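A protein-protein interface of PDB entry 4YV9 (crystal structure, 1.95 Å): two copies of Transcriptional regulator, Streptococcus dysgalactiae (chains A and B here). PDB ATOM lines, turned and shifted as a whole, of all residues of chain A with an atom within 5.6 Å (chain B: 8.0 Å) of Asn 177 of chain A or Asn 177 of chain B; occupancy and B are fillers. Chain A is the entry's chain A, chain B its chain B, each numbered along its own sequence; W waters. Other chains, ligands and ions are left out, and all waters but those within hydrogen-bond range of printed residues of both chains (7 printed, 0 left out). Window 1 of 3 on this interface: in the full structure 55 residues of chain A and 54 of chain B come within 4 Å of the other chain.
The side-chain amide nitrogen of Asn 180 of chain B is in hydrogen-bond range of the side-chain carboxylate of Glu 61 of chain A (2.8 Å).
The side-chain hydroxyl (OG) of Ser 64 of chain A sits at hydrogen-bond distance from the side-chain hydroxyl (OG) of Ser 174 of chain B (3.2 Å).
OE1 of Glu 175 of chain A is in hydrogen-bond range of NE2 of His 70 of chain B, 2.8 Å away.
The backbone carbonyl oxygen (O) of Gln 176 of chain A sits at hydrogen-bond distance from the side-chain hydroxyl (OG1) of Thr 179 of chain B (3.5 Å).
The side-chain amide oxygen (OD1) of Asn 177 of chain A lies close to the side-chain amide oxygen (OD1) of Asn 177 of chain B, 3.2 Å away.
OG1 of Thr 179 of chain A is in hydrogen-bond range of O of Gln 176 of chain B (3.1 Å).
ND2 of Asn 180 of chain A sits at hydrogen-bond distance from OE2 of Glu 61 of chain B, at 3.0 Å.
The side-chain carboxylate of Asp 60 of chain A sits close to the side-chain carboxylate of Asp 60 of chain B (3.5 Å).
The side-chain hydroxyl (OG1) of Thr 179 of chain A is in hydrogen-bond range of the side-chain amide oxygen (OD1) of Asn 177 of chain A, 2.5 Å away.
OD1 of Asp 60 of chain B is in hydrogen-bond range of OG1 of Thr 58 of chain B (2.5 Å).
The side-chain amide nitrogen (ND2) of Asn 180 of chain B sits at hydrogen-bond distance from the backbone carbonyl oxygen (O) of Ala 172 of chain B (3.5 Å).
N of Gln 176 of chain B lies close to OG of Ser 174 of chain B.
The backbone NH of Asn 177 of chain B lies within hydrogen-bond range of the side-chain hydroxyl of Ser 174 of chain B, 3.3 Å away.
The side-chain hydroxyl of Thr 179 of chain B is in hydrogen-bond range of the side-chain amide oxygen of Asn 177 of chain B (2.6 Å).
Among the printed residues, pairs that only touch across the chains: Asp 60 of chain A with Asn 177 of chain B, Ser 64 of chain A with Asn 177 of chain B, Tyr 173 of chain A with Ser 64 of chain B, Ser 174 of chain A with Ser 64 of chain B, Glu 175 of chain A with Phe 74 of chain B and Gln 176 of chain A with Phe 74 of chain B.
Of chain B, only Asn 177 comes within 4 Å of Asn 177 of chain A.
Thr 58 of chain B touches none of the printed residues of chain A.
Of the printed residues of chain A, Gln 176 of chain B touches Thr 179 (3.1 Å).
Of the printed residues of chain A, Thr 179 of chain B touches Gln 176 (3.5 Å).
Lys 181 of chain B touches none of the printed residues of chain A.
The nearest printed residue of chain B that does not touch Ser 174 of chain A is His 70 of chain B (4.8 Å).
Of the 18 printed residues of chain B, 10 touch a printed residue of chain A.
Hydrophobic or aromatic side chains of chain B that line the printed part of chain A: His 70 and Phe 74.
Asp 60 of chain A touches Asn 177 of chain B, but with the chains exchanged Asn 177 of chain A does not touch Asp 60 of chain B (4.03 Å).
Ser 64 of chain A touches Ser 174 of chain B, and with the chains exchanged Ser 174 of chain A touches Ser 64 of chain B.
Ser 64 of chain A touches Asn 177 of chain B, but with the chains exchanged Asn 177 of chain A does not touch Ser 64 of chain B (6.7 Å).
Asn 177 of chain A touches its own counterpart, Asn 177 of chain B.
Of the 14 pairs that touch across the chains among the printed residues, 8 have their exchanged pair printed and touching as well.
Water W2 lies within hydrogen-bond range of OD2 of Asp 60 of chain A (2.7 Å) and O of Asp 60 of chain B (2.8 Å).
Water W1 lies within hydrogen-bond range of the side-chain amide nitrogen of Asn 177 of chain B (2.8 Å), the side-chain hydroxyl of Thr 179 of chain B (3.2 Å) and the backbone carbonyl oxygen of Gln 176 of chain A (3.2 Å).
Water W7 bridges OG1 of Thr 179 of chain A (2.9 Å) and N of Lys 178 of chain B (2.9 Å).
Water W6 bridges OE2 of Glu 61 of chain B (2.9 Å) and ND2 of Asn 180 of chain A (3.5 Å).
Water W3 lies within hydrogen-bond range of the backbone NH (N) of Lys 178 of chain A (3.0 Å), the backbone carbonyl oxygen (O) of Gln 176 of chain A (3.2 Å) and the side-chain hydroxyl (OG1) of Thr 179 of chain B (3.2 Å).
Water W4 lies within hydrogen-bond range of OG of Ser 64 of chain A and ND2 of Asn 177 of chain B.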
ATOM      1  N   ASP A  60       8.573 -13.116   3.626  1.00  0.00           N
ATOM      2  CA  ASP A  60       7.178 -12.694   3.748  1.00  0.00           C
ATOM      3  C   ASP A  60       7.132 -11.298   4.341  1.00  0.00           C
ATOM      4  O   ASP A  60       6.489 -10.397   3.813  1.00  0.00           O
ATOM      5  CB  ASP A  60       6.374 -13.675   4.614  1.00  0.00           C
ATOM      6  CG  ASP A  60       6.174 -15.022   3.938  1.00  0.00           C
ATOM      7  OD1 ASP A  60       5.138 -15.206   3.259  1.00  0.00           O
ATOM      8  OD2 ASP A  60       7.050 -15.900   4.089  1.00  0.00           O
ATOM      9  N   GLU A  61       7.866 -11.133   5.433  1.00  0.00           N
ATOM     10  CA  GLU A  61       7.968  -9.865   6.134  1.00  0.00           C
ATOM     11  C   GLU A  61       8.600  -8.779   5.265  1.00  0.00           C
ATOM     12  O   GLU A  61       8.089  -7.670   5.191  1.00  0.00           O
ATOM     13  CB  GLU A  61       8.771 -10.075   7.421  1.00  0.00           C
ATOM     14  CG  GLU A  61       8.641  -8.984   8.445  1.00  0.00           C
ATOM     15  CD  GLU A  61       9.178  -9.439   9.791  1.00  0.00           C
ATOM     16  OE1 GLU A  61      10.405  -9.541   9.962  1.00  0.00           O
ATOM     17  OE2 GLU A  61       8.355  -9.720  10.665  1.00  0.00           O
ATOM     18  N   SER A  64       6.219  -7.488   2.725  1.00  0.00           N
ATOM     19  CA  SER A  64       5.231  -6.679   3.434  1.00  0.00           C
ATOM     20  C   SER A  64       5.696  -5.245   3.685  1.00  0.00           C
ATOM     21  O   SER A  64       4.891  -4.323   3.613  1.00  0.00           O
ATOM     22  CB  SER A  64       4.856  -7.335   4.773  1.00  0.00           C
ATOM     23  OG  SER A  64       3.799  -8.265   4.616  1.00  0.00           O
ATOM     24  N   TYR A 173       0.616 -22.490   0.421  1.00  0.00           N
ATOM     25  CA  TYR A 173       0.735 -21.504   1.491  1.00  0.00           C
ATOM     26  C   TYR A 173       1.963 -21.863   2.312  1.00  0.00           C
ATOM     27  O   TYR A 173       2.483 -22.964   2.167  1.00  0.00           O
ATOM     28  CB  TYR A 173      -0.520 -21.483   2.369  1.00  0.00           C
ATOM     29  CG  TYR A 173      -0.663 -22.705   3.251  1.00  0.00           C
ATOM     30  CD1 TYR A 173      -1.174 -23.897   2.751  1.00  0.00           C
ATOM     31  CD2 TYR A 173      -0.277 -22.670   4.588  1.00  0.00           C
ATOM     32  CE1 TYR A 173      -1.304 -25.023   3.564  1.00  0.00           C
ATOM     33  CE2 TYR A 173      -0.405 -23.779   5.402  1.00  0.00           C
ATOM     34  CZ  TYR A 173      -0.919 -24.952   4.890  1.00  0.00           C
ATOM     35  OH  TYR A 173      -1.042 -26.043   5.718  1.00  0.00           O
ATOM     36  N   SER A 174       2.433 -20.944   3.156  1.00  0.00           N
ATOM     37  CA  SER A 174       3.515 -21.256   4.101  1.00  0.00           C
ATOM     38  C   SER A 174       3.008 -21.278   5.535  1.00  0.00           C
ATOM     39  O   SER A 174       1.954 -20.716   5.837  1.00  0.00           O
ATOM     40  CB  SER A 174       4.657 -20.243   3.997  1.00  0.00           C
ATOM     41  OG  SER A 174       4.186 -18.910   4.120  1.00  0.00           O
ATOM     42  N   GLU A 175       3.765 -21.912   6.419  1.00  0.00           N
ATOM     43  CA  GLU A 175       3.432 -21.909   7.831  1.00  0.00           C
ATOM     44  C   GLU A 175       3.527 -20.506   8.406  1.00  0.00           C
ATOM     45  O   GLU A 175       2.750 -20.142   9.287  1.00  0.00           O
ATOM     46  CB  GLU A 175       4.338 -22.865   8.610  1.00  0.00           C
ATOM     47  CG  GLU A 175       4.130 -24.335   8.274  1.00  0.00           C
ATOM     48  CD  GLU A 175       4.941 -24.805   7.075  1.00  0.00           C
ATOM     49  OE1 GLU A 175       5.641 -23.973   6.457  1.00  0.00           O
ATOM     50  OE2 GLU A 175       4.881 -26.015   6.756  1.00  0.00           O
ATOM     51  N   GLN A 176       4.461 -19.713   7.891  1.00  0.00           N
ATOM     52  CA  GLN A 176       4.599 -18.328   8.328  1.00  0.00           C
ATOM     53  C   GLN A 176       3.445 -17.438   7.880  1.00  0.00           C
ATOM     54  O   GLN A 176       2.971 -16.592   8.637  1.00  0.00           O
ATOM     55  CB  GLN A 176       5.911 -17.716   7.833  1.00  0.00           C
ATOM     56  CG  GLN A 176       6.039 -16.270   8.284  1.00  0.00           C
ATOM     57  CD  GLN A 176       6.098 -16.150   9.801  1.00  0.00           C
ATOM     58  OE1 GLN A 176       5.075 -15.948  10.467  1.00  0.00           O
ATOM     59  NE2 GLN A 176       7.304 -16.218  10.349  1.00  0.00           N
ATOM     60  N   ASN A 177       2.997 -17.635   6.648  1.00  0.00           N
ATOM     61  CA  ASN A 177       1.918 -16.832   6.094  1.00  0.00           C
ATOM     62  C   ASN A 177       0.757 -17.703   5.641  1.00  0.00           C
ATOM     63  O   ASN A 177       0.783 -18.283   4.565  1.00  0.00           O
ATOM     64  CB  ASN A 177       2.427 -15.991   4.924  1.00  0.00           C
ATOM     65  CG  ASN A 177       1.412 -14.970   4.462  1.00  0.00           C
ATOM     66  OD1 ASN A 177       0.339 -14.841   5.052  1.00  0.00           O
ATOM     67  ND2 ASN A 177       1.753 -14.222   3.418  1.00  0.00           N
ATOM     68  N   LYS A 178      -0.269 -17.793   6.469  1.00  0.00           N
ATOM     69  CA  LYS A 178      -1.384 -18.656   6.151  1.00  0.00           C
ATOM     70  C   LYS A 178      -2.473 -17.916   5.413  1.00  0.00           C
ATOM     71  O   LYS A 178      -3.591 -18.409   5.319  1.00  0.00           O
ATOM     72  CB  LYS A 178      -1.942 -19.287   7.431  1.00  0.00           C
ATOM     73  CG  LYS A 178      -0.940 -20.252   8.067  1.00  0.00           C
ATOM     74  CD  LYS A 178      -1.549 -21.017   9.215  1.00  0.00           C
ATOM     75  CE  LYS A 178      -0.583 -22.051   9.745  1.00  0.00           C
ATOM     76  NZ  LYS A 178      -1.077 -22.569  11.039  1.00  0.00           N
ATOM     77  N   THR A 179      -2.147 -16.734   4.894  1.00  0.00           N
ATOM     78  CA  THR A 179      -3.128 -15.942   4.155  1.00  0.00           C
ATOM     79  C   THR A 179      -3.881 -16.769   3.122  1.00  0.00           C
ATOM     80  O   THR A 179      -5.108 -16.792   3.146  1.00  0.00           O
ATOM     81  CB  THR A 179      -2.465 -14.730   3.464  1.00  0.00           C
ATOM     82  OG1 THR A 179      -1.869 -13.897   4.466  1.00  0.00           O
ATOM     83  CG2 THR A 179      -3.502 -13.918   2.685  1.00  0.00           C
ATOM     84  N   ASN A 180      -3.170 -17.476   2.242  1.00  0.00           N
ATOM     85  CA  ASN A 180      -3.843 -18.248   1.203  1.00  0.00           C
ATOM     86  C   ASN A 180      -4.757 -19.340   1.769  1.00  0.00           C
ATOM     87  O   ASN A 180      -5.853 -19.538   1.263  1.00  0.00           O
ATOM     88  CB  ASN A 180      -2.846 -18.891   0.231  1.00  0.00           C
ATOM     89  CG  ASN A 180      -2.122 -17.862  -0.630  1.00  0.00           C
ATOM     90  OD1 ASN A 180      -2.488 -16.687  -0.641  1.00  0.00           O
ATOM     91  ND2 ASN A 180      -1.091 -18.298  -1.344  1.00  0.00           N
ATOM     92  N   THR B  58       4.235 -13.079  -5.874  1.00  0.00           N
ATOM     93  CA  THR B  58       5.191 -12.281  -5.145  1.00  0.00           C
ATOM     94  C   THR B  58       6.282 -13.226  -4.596  1.00  0.00           C
ATOM     95  O   THR B  58       6.037 -14.423  -4.409  1.00  0.00           O
ATOM     96  CB  THR B  58       4.493 -11.496  -4.047  1.00  0.00           C
ATOM     97  OG1 THR B  58       5.463 -10.945  -3.154  1.00  0.00           O
ATOM     98  CG2 THR B  58       3.533 -12.405  -3.296  1.00  0.00           C
ATOM     99  N   ASP B  60       7.575 -13.874  -1.863  1.00  0.00           N
ATOM    100  CA  ASP B  60       7.343 -14.662  -0.639  1.00  0.00           C
ATOM    101  C   ASP B  60       6.506 -15.909  -0.933  1.00  0.00           C
ATOM    102  O   ASP B  60       6.720 -16.976  -0.351  1.00  0.00           O
ATOM    103  CB  ASP B  60       6.682 -13.816   0.450  1.00  0.00           C
ATOM    104  CG  ASP B  60       5.473 -13.044  -0.048  1.00  0.00           C
ATOM    105  OD1 ASP B  60       5.588 -12.389  -1.098  1.00  0.00           O
ATOM    106  OD2 ASP B  60       4.416 -13.073   0.624  1.00  0.00           O
ATOM    107  N   GLU B  61       5.566 -15.769  -1.855  1.00  0.00           N
ATOM    108  CA  GLU B  61       4.773 -16.887  -2.355  1.00  0.00           C
ATOM    109  C   GLU B  61       5.646 -17.908  -3.107  1.00  0.00           C
ATOM    110  O   GLU B  61       5.481 -19.119  -2.957  1.00  0.00           O
ATOM    111  CB  GLU B  61       3.655 -16.346  -3.272  1.00  0.00           C
ATOM    112  CG  GLU B  61       2.365 -17.121  -3.195  1.00  0.00           C
ATOM    113  CD  GLU B  61       1.219 -16.487  -3.965  1.00  0.00           C
ATOM    114  OE1 GLU B  61       1.432 -15.589  -4.815  1.00  0.00           O
ATOM    115  OE2 GLU B  61       0.089 -16.901  -3.716  1.00  0.00           O
ATOM    116  N   SER B  64       7.841 -20.167  -0.734  1.00  0.00           N
ATOM    117  CA  SER B  64       7.195 -21.242   0.020  1.00  0.00           C
ATOM    118  C   SER B  64       6.900 -22.446  -0.874  1.00  0.00           C
ATOM    119  O   SER B  64       6.814 -23.562  -0.395  1.00  0.00           O
ATOM    120  CB  SER B  64       5.909 -20.758   0.696  1.00  0.00           C
ATOM    121  OG  SER B  64       4.789 -20.942  -0.153  1.00  0.00           O
ATOM    122  N   HIS B  70      13.028 -23.146   6.012  1.00  0.00           N
ATOM    123  CA  HIS B  70      12.706 -21.919   6.723  1.00  0.00           C
ATOM    124  C   HIS B  70      13.941 -21.310   7.371  1.00  0.00           C
ATOM    125  O   HIS B  70      15.006 -21.927   7.428  1.00  0.00           O
ATOM    126  CB  HIS B  70      11.628 -22.170   7.779  1.00  0.00           C
ATOM    127  CG  HIS B  70      10.291 -22.521   7.204  1.00  0.00           C
ATOM    128  ND1 HIS B  70       9.715 -21.812   6.171  1.00  0.00           N
ATOM    129  CD2 HIS B  70       9.407 -23.495   7.530  1.00  0.00           C
ATOM    130  CE1 HIS B  70       8.540 -22.340   5.877  1.00  0.00           C
ATOM    131  NE2 HIS B  70       8.330 -23.361   6.688  1.00  0.00           N
ATOM    132  N   PHE B  74      12.777 -19.478  12.556  1.00  0.00           N
ATOM    133  CA  PHE B  74      11.587 -20.310  12.446  1.00  0.00           C
ATOM    134  C   PHE B  74      11.938 -21.776  12.730  1.00  0.00           C
ATOM    135  O   PHE B  74      11.113 -22.537  13.246  1.00  0.00           O
ATOM    136  CB  PHE B  74      10.949 -20.165  11.058  1.00  0.00           C
ATOM    137  CG  PHE B  74       9.519 -20.623  11.002  1.00  0.00           C
ATOM    138  CD1 PHE B  74       8.493 -19.797  11.444  1.00  0.00           C
ATOM    139  CD2 PHE B  74       9.202 -21.886  10.534  1.00  0.00           C
ATOM    140  CE1 PHE B  74       7.174 -20.219  11.401  1.00  0.00           C
ATOM    141  CE2 PHE B  74       7.888 -22.315  10.484  1.00  0.00           C
ATOM    142  CZ  PHE B  74       6.872 -21.482  10.920  1.00  0.00           C
ATOM    143  N   PHE B 171       5.191  -1.614  14.582  1.00  0.00           N
ATOM    144  CA  PHE B 171       5.273  -2.900  13.895  1.00  0.00           C
ATOM    145  C   PHE B 171       4.884  -2.691  12.446  1.00  0.00           C
ATOM    146  O   PHE B 171       4.184  -1.733  12.115  1.00  0.00           O
ATOM    147  CB  PHE B 171       4.375  -3.957  14.541  1.00  0.00           C
ATOM    148  CG  PHE B 171       2.919  -3.767  14.247  1.00  0.00           C
ATOM    149  CD1 PHE B 171       2.154  -2.895  15.008  1.00  0.00           C
ATOM    150  CD2 PHE B 171       2.316  -4.449  13.199  1.00  0.00           C
ATOM    151  CE1 PHE B 171       0.808  -2.705  14.721  1.00  0.00           C
ATOM    152  CE2 PHE B 171       0.985  -4.271  12.920  1.00  0.00           C
ATOM    153  CZ  PHE B 171       0.224  -3.395  13.672  1.00  0.00           C
ATOM    154  N   ALA B 172       5.326  -3.588  11.577  1.00  0.00           N
ATOM    155  CA  ALA B 172       5.007  -3.442  10.162  1.00  0.00           C
ATOM    156  C   ALA B 172       4.085  -4.550   9.682  1.00  0.00           C
ATOM    157  O   ALA B 172       4.303  -5.724   9.990  1.00  0.00           O
ATOM    158  CB  ALA B 172       6.278  -3.418   9.333  1.00  0.00           C
ATOM    159  N   TYR B 173       3.050  -4.170   8.937  1.00  0.00           N
ATOM    160  CA  TYR B 173       2.235  -5.151   8.230  1.00  0.00           C
ATOM    161  C   TYR B 173       1.788  -4.619   6.885  1.00  0.00           C
ATOM    162  O   TYR B 173       1.955  -3.437   6.584  1.00  0.00           O
ATOM    163  CB  TYR B 173       1.013  -5.562   9.059  1.00  0.00           C
ATOM    164  CG  TYR B 173      -0.113  -4.549   9.127  1.00  0.00           C
ATOM    165  CD1 TYR B 173      -0.038  -3.451   9.974  1.00  0.00           C
ATOM    166  CD2 TYR B 173      -1.270  -4.711   8.370  1.00  0.00           C
ATOM    167  CE1 TYR B 173      -1.083  -2.529  10.059  1.00  0.00           C
ATOM    168  CE2 TYR B 173      -2.313  -3.791   8.439  1.00  0.00           C
ATOM    169  CZ  TYR B 173      -2.213  -2.704   9.288  1.00  0.00           C
ATOM    170  OH  TYR B 173      -3.244  -1.792   9.374  1.00  0.00           O
ATOM    171  N   SER B 174       1.220  -5.495   6.068  1.00  0.00           N
ATOM    172  CA  SER B 174       0.598  -5.051   4.830  1.00  0.00           C
ATOM    173  C   SER B 174      -0.806  -5.607   4.748  1.00  0.00           C
ATOM    174  O   SER B 174      -1.187  -6.480   5.529  1.00  0.00           O
ATOM    175  CB  SER B 174       1.405  -5.493   3.606  1.00  0.00           C
ATOM    176  OG  SER B 174       1.228  -6.877   3.353  1.00  0.00           O
ATOM    177  N   GLU B 175      -1.558  -5.112   3.777  1.00  0.00           N
ATOM    178  CA  GLU B 175      -2.910  -5.571   3.551  1.00  0.00           C
ATOM    179  C   GLU B 175      -2.915  -7.074   3.236  1.00  0.00           C
ATOM    180  O   GLU B 175      -3.859  -7.781   3.581  1.00  0.00           O
ATOM    181  CB  GLU B 175      -3.559  -4.755   2.423  1.00  0.00           C
ATOM    182  CG  GLU B 175      -3.364  -3.229   2.569  1.00  0.00           C
ATOM    183  CD  GLU B 175      -3.790  -2.416   1.327  1.00  0.00           C
ATOM    184  OE1 GLU B 175      -4.577  -2.926   0.497  1.00  0.00           O
ATOM    185  OE2 GLU B 175      -3.340  -1.255   1.179  1.00  0.00           O
ATOM    186  N   GLN B 176      -1.853  -7.565   2.599  1.00  0.00           N
ATOM    187  CA  GLN B 176      -1.809  -8.966   2.178  1.00  0.00           C
ATOM    188  C   GLN B 176      -1.339  -9.917   3.252  1.00  0.00           C
ATOM    189  O   GLN B 176      -1.492 -11.127   3.105  1.00  0.00           O
ATOM    190  CB  GLN B 176      -0.898  -9.153   0.958  1.00  0.00           C
ATOM    191  CG  GLN B 176      -1.566  -8.809  -0.347  1.00  0.00           C
ATOM    192  CD  GLN B 176      -1.754  -7.322  -0.521  1.00  0.00           C
ATOM    193  OE1 GLN B 176      -0.901  -6.528  -0.120  1.00  0.00           O
ATOM    194  NE2 GLN B 176      -2.880  -6.933  -1.104  1.00  0.00           N
ATOM    195  N   ASN B 177      -0.741  -9.382   4.311  1.00  0.00           N
ATOM    196  CA  ASN B 177      -0.181 -10.220   5.359  1.00  0.00           C
ATOM    197  C   ASN B 177      -0.309  -9.578   6.743  1.00  0.00           C
ATOM    198  O   ASN B 177       0.482  -8.714   7.120  1.00  0.00           O
ATOM    199  CB  ASN B 177       1.286 -10.529   5.050  1.00  0.00           C
ATOM    200  CG  ASN B 177       1.838 -11.639   5.923  1.00  0.00           C
ATOM    201  OD1 ASN B 177       1.102 -12.245   6.707  1.00  0.00           O
ATOM    202  ND2 ASN B 177       3.135 -11.919   5.788  1.00  0.00           N
ATOM    203  N   LYS B 178      -1.310 -10.000   7.499  1.00  0.00           N
ATOM    204  CA  LYS B 178      -1.543  -9.414   8.807  1.00  0.00           C
ATOM    205  C   LYS B 178      -1.015 -10.283   9.933  1.00  0.00           C
ATOM    206  O   LYS B 178      -1.443 -10.163  11.081  1.00  0.00           O
ATOM    207  CB  LYS B 178      -3.024  -9.130   8.976  1.00  0.00           C
ATOM    208  CG  LYS B 178      -3.422  -7.948   8.089  1.00  0.00           C
ATOM    209  CD  LYS B 178      -4.889  -7.895   7.878  1.00  0.00           C
ATOM    210  CE  LYS B 178      -5.271  -6.638   7.135  1.00  0.00           C
ATOM    211  NZ  LYS B 178      -6.699  -6.748   6.798  1.00  0.00           N
ATOM    212  N   THR B 179      -0.057 -11.137   9.595  1.00  0.00           N
ATOM    213  CA  THR B 179       0.526 -12.036  10.572  1.00  0.00           C
ATOM    214  C   THR B 179       1.062 -11.249  11.756  1.00  0.00           C
ATOM    215  O   THR B 179       0.704 -11.539  12.891  1.00  0.00           O
ATOM    216  CB  THR B 179       1.641 -12.886   9.952  1.00  0.00           C
ATOM    217  OG1 THR B 179       1.085 -13.661   8.884  1.00  0.00           O
ATOM    218  CG2 THR B 179       2.223 -13.826  10.984  1.00  0.00           C
ATOM    219  N   ASN B 180       1.885 -10.233  11.505  1.00  0.00           N
ATOM    220  CA  ASN B 180       2.441  -9.489  12.637  1.00  0.00           C
ATOM    221  C   ASN B 180       1.390  -8.674  13.390  1.00  0.00           C
ATOM    222  O   ASN B 180       1.509  -8.476  14.592  1.00  0.00           O
ATOM    223  CB  ASN B 180       3.572  -8.565  12.199  1.00  0.00           C
ATOM    224  CG  ASN B 180       4.808  -9.330  11.804  1.00  0.00           C
ATOM    225  OD1 ASN B 180       4.868 -10.551  11.980  1.00  0.00           O
ATOM    226  ND2 ASN B 180       5.795  -8.630  11.241  1.00  0.00           N
ATOM    227  N   LYS B 181       0.375  -8.197  12.684  1.00  0.00           N
ATOM    228  CA  LYS B 181      -0.674  -7.401  13.318  1.00  0.00           C
ATOM    229  C   LYS B 181      -1.490  -8.262  14.281  1.00  0.00           C
ATOM    230  O   LYS B 181      -1.835  -7.849  15.397  1.00  0.00           O
ATOM    231  CB  LYS B 181      -1.574  -6.772  12.248  1.00  0.00           C
ATOM    232  CG  LYS B 181      -2.653  -5.878  12.816  1.00  0.00           C
ATOM    233  CD  LYS B 181      -3.535  -5.307  11.724  1.00  0.00           C
ATOM    234  CE  LYS B 181      -4.571  -4.348  12.305  1.00  0.00           C
ATOM    235  NZ  LYS B 181      -5.341  -3.629  11.231  1.00  0.00           N
ATOM    236  N   THR B 182      -1.797  -9.475  13.850  1.00  0.00           N
ATOM    237  CA  THR B 182      -2.541 -10.384  14.710  1.00  0.00           C
ATOM    238  C   THR B 182      -1.723 -10.719  15.968  1.00  0.00           C
ATOM    239  O   THR B 182      -2.251 -10.690  17.095  1.00  0.00           O
ATOM    240  CB  THR B 182      -2.942 -11.646  13.920  1.00  0.00           C
ATOM    241  OG1 THR B 182      -3.912 -11.267  12.934  1.00  0.00           O
ATOM    242  CG2 THR B 182      -3.570 -12.684  14.818  1.00  0.00           C
HETATM  243  O   HOH W   1       4.034 -13.705   7.697  1.00  0.00           O
HETATM  244  O   HOH W   2       7.537 -17.741   2.177  1.00  0.00           O
HETATM  245  O   HOH W   3      -0.164 -16.606   9.219  1.00  0.00           O
HETATM  246  O   HOH W   4       5.010  -9.524   7.434  1.00  0.00           O
HETATM  247  O   HOH W   5       4.282 -11.084   2.784  1.00  0.00           O
HETATM  248  O   HOH W   6       0.903 -19.735  -3.807  1.00  0.00           O
HETATM  249  O   HOH W   7      -3.111 -11.932   6.189  1.00  0.00           O
